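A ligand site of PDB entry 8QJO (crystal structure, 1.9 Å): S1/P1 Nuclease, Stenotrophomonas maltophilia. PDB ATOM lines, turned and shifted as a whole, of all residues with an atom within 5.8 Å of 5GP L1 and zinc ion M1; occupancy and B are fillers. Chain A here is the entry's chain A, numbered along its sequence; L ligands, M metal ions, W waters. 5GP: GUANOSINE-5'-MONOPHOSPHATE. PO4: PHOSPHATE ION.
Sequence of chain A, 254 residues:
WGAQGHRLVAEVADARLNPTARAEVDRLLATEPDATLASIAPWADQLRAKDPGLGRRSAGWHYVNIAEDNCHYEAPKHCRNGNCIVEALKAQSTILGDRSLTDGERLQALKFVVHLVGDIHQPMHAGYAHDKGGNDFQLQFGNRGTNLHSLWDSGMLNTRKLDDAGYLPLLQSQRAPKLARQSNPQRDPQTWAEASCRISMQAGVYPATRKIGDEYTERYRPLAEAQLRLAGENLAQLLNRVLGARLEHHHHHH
The nearest printed residue that does not touch zinc ion M1 is Trp 1 (4.04 Å).
Water W1 bridges an oxygen (O6) of 5GP L1 (2.8 Å) and the side-chain hydroxyl of Tyr 63 (3.1 Å).
Water W2 lies within hydrogen-bond range of NH1 of Arg 48 (2.7 Å), O of Ala 59 (2.8 Å) and O2' of 5GP L1 (3.0 Å).
An oxygen (O4') of 5GP L1 is in hydrogen-bond range of the side-chain amide nitrogen (ND2) of Asn 135 (2.6 Å).
N1 of 5GP L1 lies within hydrogen-bond range of OD1 of Asn 65.
A nitrogen (N2) of 5GP L1 is in hydrogen-bond range of the backbone carbonyl oxygen (O) of Met 124, at 2.9 Å.
O1P of 5GP L1 is in salt-bridge range of NE of Arg 48 (3.9 Å).
Zinc ion M1 is bound by O2 of PO4 L2, NE2 of His 125, NE2 of His 149, O3' of 5GP L1, OD2 of Asp 153 and OD1 of Asp 153.
Zinc ion M1 has six donor atoms within binding distance.
A nitrogen (N1) of 5GP L1 sits close to the backbone NH (N) of Gly 133.
Merely in contact with 5GP L1: Lys 132, Tyr 63 and His 62.
Hydrophobic or aromatic side chains within 4 Å of 5GP L1: His 62, Tyr 63, His 125 and His 149.
11 residues have an atom within 4 Å of 5GP L1: Arg 48, His 62, Tyr 63, Asn 65, Met 124, His 125, Lys 132, Gly 133, Asn 135, His 149 and Asp 153.
The nearest printed residue that does not touch 5GP L1 is Gly 127 (4.2 Å).
ND1 of His 125 sits at hydrogen-bond distance from O of His 62 (2.7 Å).
O of His 125 is in hydrogen-bond range of N of Val 64, at 2.9 Å.
O of Gly 133 lies within hydrogen-bond range of ND1 of His 149 (2.7 Å).
The side-chain amide nitrogen of Gln 122 sits close to the backbone NH of Asp 153.
ND2 of Asn 135 is in hydrogen-bond range of O of Lys 132 (3.0 Å).
The backbone carbonyl oxygen (O) of Tyr 128 sits close to the side-chain amide oxygen (OD1) of Asn 65 (3.5 Å).
The backbone NH (N) of Gly 133 sits at hydrogen-bond distance from the backbone carbonyl oxygen (O) of Tyr 128, at 2.8 Å.
ND1 of His 62 sits close to NH1 of Arg 48.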
ATOM      1  N   TRP A   1       4.756 -23.673 -30.383  1.00  0.00           N
ATOM      2  CA  TRP A   1       5.582 -24.009 -31.557  1.00  0.00           C
ATOM      3  C   TRP A   1       4.940 -25.160 -32.347  1.00  0.00           C
ATOM      4  O   TRP A   1       4.196 -25.930 -31.756  1.00  0.00           O
ATOM      5  CB  TRP A   1       7.038 -24.375 -31.168  1.00  0.00           C
ATOM      6  CG  TRP A   1       7.681 -23.426 -30.218  1.00  0.00           C
ATOM      7  CD1 TRP A   1       7.851 -23.588 -28.873  1.00  0.00           C
ATOM      8  CD2 TRP A   1       8.202 -22.117 -30.526  1.00  0.00           C
ATOM      9  NE1 TRP A   1       8.424 -22.472 -28.329  1.00  0.00           N
ATOM     10  CE2 TRP A   1       8.681 -21.556 -29.327  1.00  0.00           C
ATOM     11  CE3 TRP A   1       8.341 -21.390 -31.711  1.00  0.00           C
ATOM     12  CZ2 TRP A   1       9.247 -20.297 -29.253  1.00  0.00           C
ATOM     13  CZ3 TRP A   1       8.920 -20.140 -31.653  1.00  0.00           C
ATOM     14  CH2 TRP A   1       9.359 -19.597 -30.441  1.00  0.00           C
ATOM     15  N   ASP A  45       0.251 -31.920 -28.567  1.00  0.00           N
ATOM     16  CA  ASP A  45      -0.490 -31.330 -29.727  1.00  0.00           C
ATOM     17  C   ASP A  45      -1.228 -32.441 -30.488  1.00  0.00           C
ATOM     18  O   ASP A  45      -2.336 -32.169 -30.949  1.00  0.00           O
ATOM     19  CB  ASP A  45       0.401 -30.563 -30.705  1.00  0.00           C
ATOM     20  CG  ASP A  45       0.913 -29.243 -30.174  1.00  0.00           C
ATOM     21  OD1 ASP A  45       0.269 -28.678 -29.221  1.00  0.00           O
ATOM     22  OD2 ASP A  45       1.952 -28.793 -30.710  1.00  0.00           O
ATOM     23  N   ARG A  48      -4.149 -33.350 -28.237  1.00  0.00           N
ATOM     24  CA  ARG A  48      -5.180 -32.299 -28.444  1.00  0.00           C
ATOM     25  C   ARG A  48      -5.984 -32.591 -29.722  1.00  0.00           C
ATOM     26  O   ARG A  48      -7.197 -32.434 -29.703  1.00  0.00           O
ATOM     27  CB  ARG A  48      -4.566 -30.898 -28.571  1.00  0.00           C
ATOM     28  CG  ARG A  48      -5.610 -29.796 -28.649  1.00  0.00           C
ATOM     29  CD  ARG A  48      -5.043 -28.405 -28.865  1.00  0.00           C
ATOM     30  NE  ARG A  48      -4.101 -28.386 -29.986  1.00  0.00           N
ATOM     31  CZ  ARG A  48      -2.984 -27.681 -30.051  1.00  0.00           C
ATOM     32  NH1 ARG A  48      -2.596 -26.844 -29.070  1.00  0.00           N
ATOM     33  NH2 ARG A  48      -2.244 -27.803 -31.143  1.00  0.00           N
ATOM     34  N   ALA A  59      -6.647 -28.672 -23.968  1.00  0.00           N
ATOM     35  CA  ALA A  59      -6.387 -27.700 -25.054  1.00  0.00           C
ATOM     36  C   ALA A  59      -5.962 -26.363 -24.454  1.00  0.00           C
ATOM     37  O   ALA A  59      -4.969 -25.796 -24.929  1.00  0.00           O
ATOM     38  CB  ALA A  59      -7.588 -27.498 -25.963  1.00  0.00           C
ATOM     39  N   HIS A  62      -2.170 -25.130 -23.238  1.00  0.00           N
ATOM     40  CA  HIS A  62      -1.064 -24.730 -24.168  1.00  0.00           C
ATOM     41  C   HIS A  62      -0.785 -23.240 -24.097  1.00  0.00           C
ATOM     42  O   HIS A  62       0.283 -22.810 -24.584  1.00  0.00           O
ATOM     43  CB  HIS A  62      -1.339 -25.209 -25.602  1.00  0.00           C
ATOM     44  CG  HIS A  62      -1.373 -26.711 -25.706  1.00  0.00           C
ATOM     45  ND1 HIS A  62      -0.509 -27.427 -26.482  1.00  0.00           N
ATOM     46  CD2 HIS A  62      -2.173 -27.613 -25.098  1.00  0.00           C
ATOM     47  CE1 HIS A  62      -0.788 -28.705 -26.366  1.00  0.00           C
ATOM     48  NE2 HIS A  62      -1.810 -28.854 -25.523  1.00  0.00           N
ATOM     49  N   TYR A  63      -1.673 -22.448 -23.503  1.00  0.00           N
ATOM     50  CA  TYR A  63      -1.583 -20.978 -23.584  1.00  0.00           C
ATOM     51  C   TYR A  63      -2.178 -20.322 -22.345  1.00  0.00           C
ATOM     52  O   TYR A  63      -2.747 -20.979 -21.440  1.00  0.00           O
ATOM     53  CB  TYR A  63      -2.233 -20.489 -24.892  1.00  0.00           C
ATOM     54  CG  TYR A  63      -3.702 -20.794 -24.978  1.00  0.00           C
ATOM     55  CD1 TYR A  63      -4.639 -19.983 -24.347  1.00  0.00           C
ATOM     56  CD2 TYR A  63      -4.153 -21.919 -25.643  1.00  0.00           C
ATOM     57  CE1 TYR A  63      -5.996 -20.263 -24.407  1.00  0.00           C
ATOM     58  CE2 TYR A  63      -5.506 -22.212 -25.698  1.00  0.00           C
ATOM     59  CZ  TYR A  63      -6.430 -21.378 -25.082  1.00  0.00           C
ATOM     60  OH  TYR A  63      -7.756 -21.685 -25.138  1.00  0.00           O
ATOM     61  N   VAL A  64      -1.997 -19.004 -22.278  1.00  0.00           N
ATOM     62  CA  VAL A  64      -2.672 -18.137 -21.294  1.00  0.00           C
ATOM     63  C   VAL A  64      -2.798 -16.727 -21.893  1.00  0.00           C
ATOM     64  O   VAL A  64      -1.810 -16.212 -22.440  1.00  0.00           O
ATOM     65  CB  VAL A  64      -1.931 -18.156 -19.958  1.00  0.00           C
ATOM     66  CG1 VAL A  64      -0.596 -17.425 -19.990  1.00  0.00           C
ATOM     67  CG2 VAL A  64      -2.812 -17.602 -18.851  1.00  0.00           C
ATOM     68  N   ASN A  65      -3.971 -16.118 -21.783  1.00  0.00           N
ATOM     69  CA  ASN A  65      -4.260 -14.807 -22.411  1.00  0.00           C
ATOM     70  C   ASN A  65      -4.099 -13.736 -21.331  1.00  0.00           C
ATOM     71  O   ASN A  65      -4.979 -13.642 -20.504  1.00  0.00           O
ATOM     72  CB  ASN A  65      -5.646 -14.763 -23.052  1.00  0.00           C
ATOM     73  CG  ASN A  65      -5.791 -15.763 -24.171  1.00  0.00           C
ATOM     74  OD1 ASN A  65      -4.890 -15.901 -25.007  1.00  0.00           O
ATOM     75  ND2 ASN A  65      -6.919 -16.457 -24.215  1.00  0.00           N
ATOM     76  N   ASP A 119       6.015 -24.295 -25.277  1.00  0.00           N
ATOM     77  CA  ASP A 119       4.890 -23.385 -25.561  1.00  0.00           C
ATOM     78  C   ASP A 119       4.956 -22.132 -24.694  1.00  0.00           C
ATOM     79  O   ASP A 119       4.636 -21.091 -25.205  1.00  0.00           O
ATOM     80  CB  ASP A 119       3.544 -24.081 -25.381  1.00  0.00           C
ATOM     81  CG  ASP A 119       3.081 -24.840 -26.637  1.00  0.00           C
ATOM     82  OD1 ASP A 119       3.782 -24.771 -27.670  1.00  0.00           O
ATOM     83  OD2 ASP A 119       2.027 -25.476 -26.555  1.00  0.00           O
ATOM     84  N   GLN A 122       6.801 -19.394 -26.326  1.00  0.00           N
ATOM     85  CA  GLN A 122       6.316 -18.864 -27.619  1.00  0.00           C
ATOM     86  C   GLN A 122       5.521 -17.608 -27.276  1.00  0.00           C
ATOM     87  O   GLN A 122       4.488 -17.686 -26.600  1.00  0.00           O
ATOM     88  CB  GLN A 122       5.547 -19.951 -28.370  1.00  0.00           C
ATOM     89  CG  GLN A 122       5.568 -19.867 -29.896  1.00  0.00           C
ATOM     90  CD  GLN A 122       4.682 -18.778 -30.445  1.00  0.00           C
ATOM     91  OE1 GLN A 122       4.894 -17.606 -30.177  1.00  0.00           O
ATOM     92  NE2 GLN A 122       3.654 -19.162 -31.213  1.00  0.00           N
ATOM     93  N   MET A 124       3.285 -15.708 -28.594  1.00  0.00           N
ATOM     94  CA  MET A 124       1.859 -15.661 -28.952  1.00  0.00           C
ATOM     95  C   MET A 124       1.045 -16.611 -28.049  1.00  0.00           C
ATOM     96  O   MET A 124      -0.180 -16.453 -27.950  1.00  0.00           O
ATOM     97  CB  MET A 124       1.654 -15.982 -30.432  1.00  0.00           C
ATOM     98  CG  MET A 124       2.426 -15.024 -31.338  1.00  0.00           C
ATOM     99  SD  MET A 124       2.129 -13.231 -31.049  1.00  0.00           S
ATOM    100  CE  MET A 124       0.373 -13.187 -31.336  1.00  0.00           C
ATOM    101  N   HIS A 125       1.700 -17.539 -27.360  1.00  0.00           N
ATOM    102  CA  HIS A 125       1.057 -18.431 -26.356  1.00  0.00           C
ATOM    103  C   HIS A 125       0.743 -17.679 -25.038  1.00  0.00           C
ATOM    104  O   HIS A 125       0.159 -18.289 -24.101  1.00  0.00           O
ATOM    105  CB  HIS A 125       1.908 -19.671 -26.189  1.00  0.00           C
ATOM    106  CG  HIS A 125       1.670 -20.692 -27.251  1.00  0.00           C
ATOM    107  ND1 HIS A 125       1.182 -21.949 -26.962  1.00  0.00           N
ATOM    108  CD2 HIS A 125       1.888 -20.684 -28.590  1.00  0.00           C
ATOM    109  CE1 HIS A 125       1.076 -22.641 -28.079  1.00  0.00           C
ATOM    110  NE2 HIS A 125       1.495 -21.900 -29.081  1.00  0.00           N
ATOM    111  N   ALA A 126       1.120 -16.403 -24.908  1.00  0.00           N
ATOM    112  CA  ALA A 126       0.851 -15.599 -23.688  1.00  0.00           C
ATOM    113  C   ALA A 126       0.260 -14.247 -24.084  1.00  0.00           C
ATOM    114  O   ALA A 126       0.338 -13.319 -23.270  1.00  0.00           O
ATOM    115  CB  ALA A 126       2.099 -15.447 -22.873  1.00  0.00           C
ATOM    116  N   GLY A 127      -0.337 -14.148 -25.273  1.00  0.00           N
ATOM    117  CA  GLY A 127      -0.802 -12.891 -25.899  1.00  0.00           C
ATOM    118  C   GLY A 127      -2.252 -12.556 -25.575  1.00  0.00           C
ATOM    119  O   GLY A 127      -2.676 -12.684 -24.430  1.00  0.00           O
ATOM    120  N   TYR A 128      -2.995 -12.079 -26.588  1.00  0.00           N
ATOM    121  CA  TYR A 128      -4.362 -11.523 -26.433  1.00  0.00           C
ATOM    122  C   TYR A 128      -5.427 -12.618 -26.551  1.00  0.00           C
ATOM    123  O   TYR A 128      -5.368 -13.470 -27.462  1.00  0.00           O
ATOM    124  CB  TYR A 128      -4.618 -10.446 -27.493  1.00  0.00           C
ATOM    125  CG  TYR A 128      -3.833  -9.172 -27.309  1.00  0.00           C
ATOM    126  CD1 TYR A 128      -4.329  -8.130 -26.539  1.00  0.00           C
ATOM    127  CD2 TYR A 128      -2.586  -9.009 -27.895  1.00  0.00           C
ATOM    128  CE1 TYR A 128      -3.625  -6.944 -26.366  1.00  0.00           C
ATOM    129  CE2 TYR A 128      -1.869  -7.832 -27.737  1.00  0.00           C
ATOM    130  CZ  TYR A 128      -2.390  -6.806 -26.967  1.00  0.00           C
ATOM    131  OH  TYR A 128      -1.687  -5.656 -26.780  1.00  0.00           O
ATOM    132  N   ALA A 129      -6.367 -12.607 -25.613  1.00  0.00           N
ATOM    133  CA  ALA A 129      -7.662 -13.298 -25.749  1.00  0.00           C
ATOM    134  C   ALA A 129      -8.394 -12.800 -26.998  1.00  0.00           C
ATOM    135  O   ALA A 129      -9.064 -13.604 -27.657  1.00  0.00           O
ATOM    136  CB  ALA A 129      -8.469 -13.061 -24.495  1.00  0.00           C
ATOM    137  N   LYS A 132      -7.212 -14.483 -30.029  1.00  0.00           N
ATOM    138  CA  LYS A 132      -6.839 -15.886 -29.650  1.00  0.00           C
ATOM    139  C   LYS A 132      -5.347 -16.139 -29.918  1.00  0.00           C
ATOM    140  O   LYS A 132      -5.008 -17.025 -30.696  1.00  0.00           O
ATOM    141  CB  LYS A 132      -7.699 -16.910 -30.380  1.00  0.00           C
ATOM    142  CG  LYS A 132      -9.196 -16.661 -30.246  1.00  0.00           C
ATOM    143  CD  LYS A 132     -10.049 -17.916 -30.227  1.00  0.00           C
ATOM    144  CE  LYS A 132      -9.448 -19.085 -30.988  1.00  0.00           C
ATOM    145  NZ  LYS A 132     -10.493 -20.022 -31.496  1.00  0.00           N
ATOM    146  N   GLY A 133      -4.470 -15.387 -29.278  1.00  0.00           N
ATOM    147  CA  GLY A 133      -3.021 -15.587 -29.406  1.00  0.00           C
ATOM    148  C   GLY A 133      -2.527 -15.375 -30.823  1.00  0.00           C
ATOM    149  O   GLY A 133      -1.578 -16.034 -31.177  1.00  0.00           O
ATOM    150  N   GLY A 134      -3.194 -14.543 -31.611  1.00  0.00           N
ATOM    151  CA  GLY A 134      -2.784 -14.152 -32.976  1.00  0.00           C
ATOM    152  C   GLY A 134      -3.391 -15.030 -34.051  1.00  0.00           C
ATOM    153  O   GLY A 134      -3.132 -14.759 -35.230  1.00  0.00           O
ATOM    154  N   ASN A 135      -4.156 -16.058 -33.691  1.00  0.00           N
ATOM    155  CA  ASN A 135      -4.826 -16.937 -34.686  1.00  0.00           C
ATOM    156  C   ASN A 135      -5.772 -16.122 -35.576  1.00  0.00           C
ATOM    157  O   ASN A 135      -5.845 -16.409 -36.768  1.00  0.00           O
ATOM    158  CB  ASN A 135      -5.557 -18.097 -34.025  1.00  0.00           C
ATOM    159  CG  ASN A 135      -4.597 -19.204 -33.686  1.00  0.00           C
ATOM    160  OD1 ASN A 135      -4.030 -19.814 -34.579  1.00  0.00           O
ATOM    161  ND2 ASN A 135      -4.352 -19.406 -32.395  1.00  0.00           N
ATOM    162  N   HIS A 149      -0.163 -16.196 -35.244  1.00  0.00           N
ATOM    163  CA  HIS A 149       0.147 -17.344 -34.344  1.00  0.00           C
ATOM    164  C   HIS A 149       1.017 -18.351 -35.098  1.00  0.00           C
ATOM    165  O   HIS A 149       2.083 -18.715 -34.585  1.00  0.00           O
ATOM    166  CB  HIS A 149      -1.103 -18.005 -33.747  1.00  0.00           C
ATOM    167  CG  HIS A 149      -0.741 -18.971 -32.661  1.00  0.00           C
ATOM    168  ND1 HIS A 149      -0.749 -18.604 -31.326  1.00  0.00           N
ATOM    169  CD2 HIS A 149      -0.316 -20.253 -32.715  1.00  0.00           C
ATOM    170  CE1 HIS A 149      -0.401 -19.649 -30.592  1.00  0.00           C
ATOM    171  NE2 HIS A 149      -0.068 -20.658 -31.417  1.00  0.00           N
ATOM    172  N   ASP A 153       4.710 -19.892 -34.446  1.00  0.00           N
ATOM    173  CA  ASP A 153       4.772 -21.360 -34.244  1.00  0.00           C
ATOM    174  C   ASP A 153       5.796 -22.001 -35.166  1.00  0.00           C
ATOM    175  O   ASP A 153       6.596 -22.841 -34.659  1.00  0.00           O
ATOM    176  CB  ASP A 153       3.411 -22.056 -34.397  1.00  0.00           C
ATOM    177  CG  ASP A 153       2.626 -22.139 -33.105  1.00  0.00           C
ATOM    178  OD1 ASP A 153       3.207 -21.756 -32.014  1.00  0.00           O
ATOM    179  OD2 ASP A 153       1.489 -22.658 -33.164  1.00  0.00           O
HETATM  180  P   5GP L   1      -6.068 -24.254 -32.424  1.00  0.00           P
HETATM  181  O1P 5GP L   1      -5.317 -25.559 -32.336  1.00  0.00           O
HETATM  182  O2P 5GP L   1      -6.599 -23.841 -33.797  1.00  0.00           O
HETATM  183  O3P 5GP L   1      -7.183 -24.135 -31.346  1.00  0.00           O
HETATM  184  O5' 5GP L   1      -4.984 -23.047 -32.039  1.00  0.00           O
HETATM  185  C5' 5GP L   1      -3.767 -22.900 -32.773  1.00  0.00           C
HETATM  186  C4' 5GP L   1      -2.705 -22.463 -31.803  1.00  0.00           C
HETATM  187  O4' 5GP L   1      -3.175 -21.304 -31.088  1.00  0.00           O
HETATM  188  C3' 5GP L   1      -2.273 -23.486 -30.746  1.00  0.00           C
HETATM  189  O3' 5GP L   1      -0.861 -23.441 -30.558  1.00  0.00           O
HETATM  190  C2' 5GP L   1      -3.112 -23.089 -29.521  1.00  0.00           C
HETATM  191  O2' 5GP L   1      -2.456 -23.349 -28.285  1.00  0.00           O
HETATM  192  C1' 5GP L   1      -3.216 -21.570 -29.692  1.00  0.00           C
HETATM  193  N9  5GP L   1      -4.436 -20.952 -29.166  1.00  0.00           N
HETATM  194  C8  5GP L   1      -5.769 -21.289 -29.340  1.00  0.00           C
HETATM  195  N7  5GP L   1      -6.604 -20.402 -28.818  1.00  0.00           N
HETATM  196  C5  5GP L   1      -5.765 -19.462 -28.229  1.00  0.00           C
HETATM  197  C6  5GP L   1      -6.052 -18.359 -27.391  1.00  0.00           C
HETATM  198  O6  5GP L   1      -7.164 -18.008 -27.002  1.00  0.00           O
HETATM  199  N1  5GP L   1      -4.910 -17.748 -26.910  1.00  0.00           N
HETATM  200  C2  5GP L   1      -3.609 -18.136 -27.214  1.00  0.00           C
HETATM  201  N2  5GP L   1      -2.616 -17.414 -26.656  1.00  0.00           N
HETATM  202  N3  5GP L   1      -3.321 -19.179 -28.000  1.00  0.00           N
HETATM  203  C4  5GP L   1      -4.420 -19.783 -28.459  1.00  0.00           C
HETATM  204  P   PO4 L   2       0.898 -25.590 -30.197  1.00  0.00           P
HETATM  205  O1  PO4 L   2       0.212 -26.244 -31.384  1.00  0.00           O
HETATM  206  O2  PO4 L   2       1.362 -24.233 -30.602  1.00  0.00           O
HETATM  207  O3  PO4 L   2       2.121 -26.436 -29.789  1.00  0.00           O
HETATM  208  O4  PO4 L   2      -0.034 -25.505 -29.040  1.00  0.00           O
HETATM  209 ZN    ZN M   1       0.980 -22.355 -30.977  1.00  0.00          ZN
HETATM  210 ZN    ZN M   2       3.815 -25.519 -29.659  1.00  0.00          ZN
HETATM  211 ZN    ZN M   3       1.110 -26.911 -27.743  1.00  0.00          ZN
HETATM  212  O   HOH W   1      -9.433 -19.185 -25.942  1.00  0.00           O
HETATM  213  O   HOH W   2      -4.476 -25.471 -27.661  1.00  0.00           O
HETATM  214  O   HOH W   3      -0.916 -24.529 -33.541  1.00  0.00           O
HETATM  215  O   HOH W   4      -8.339 -26.397 -35.236  1.00  0.00           O
HETATM  216  O   HOH W   5      -6.695 -24.870 -28.709  1.00  0.00           O
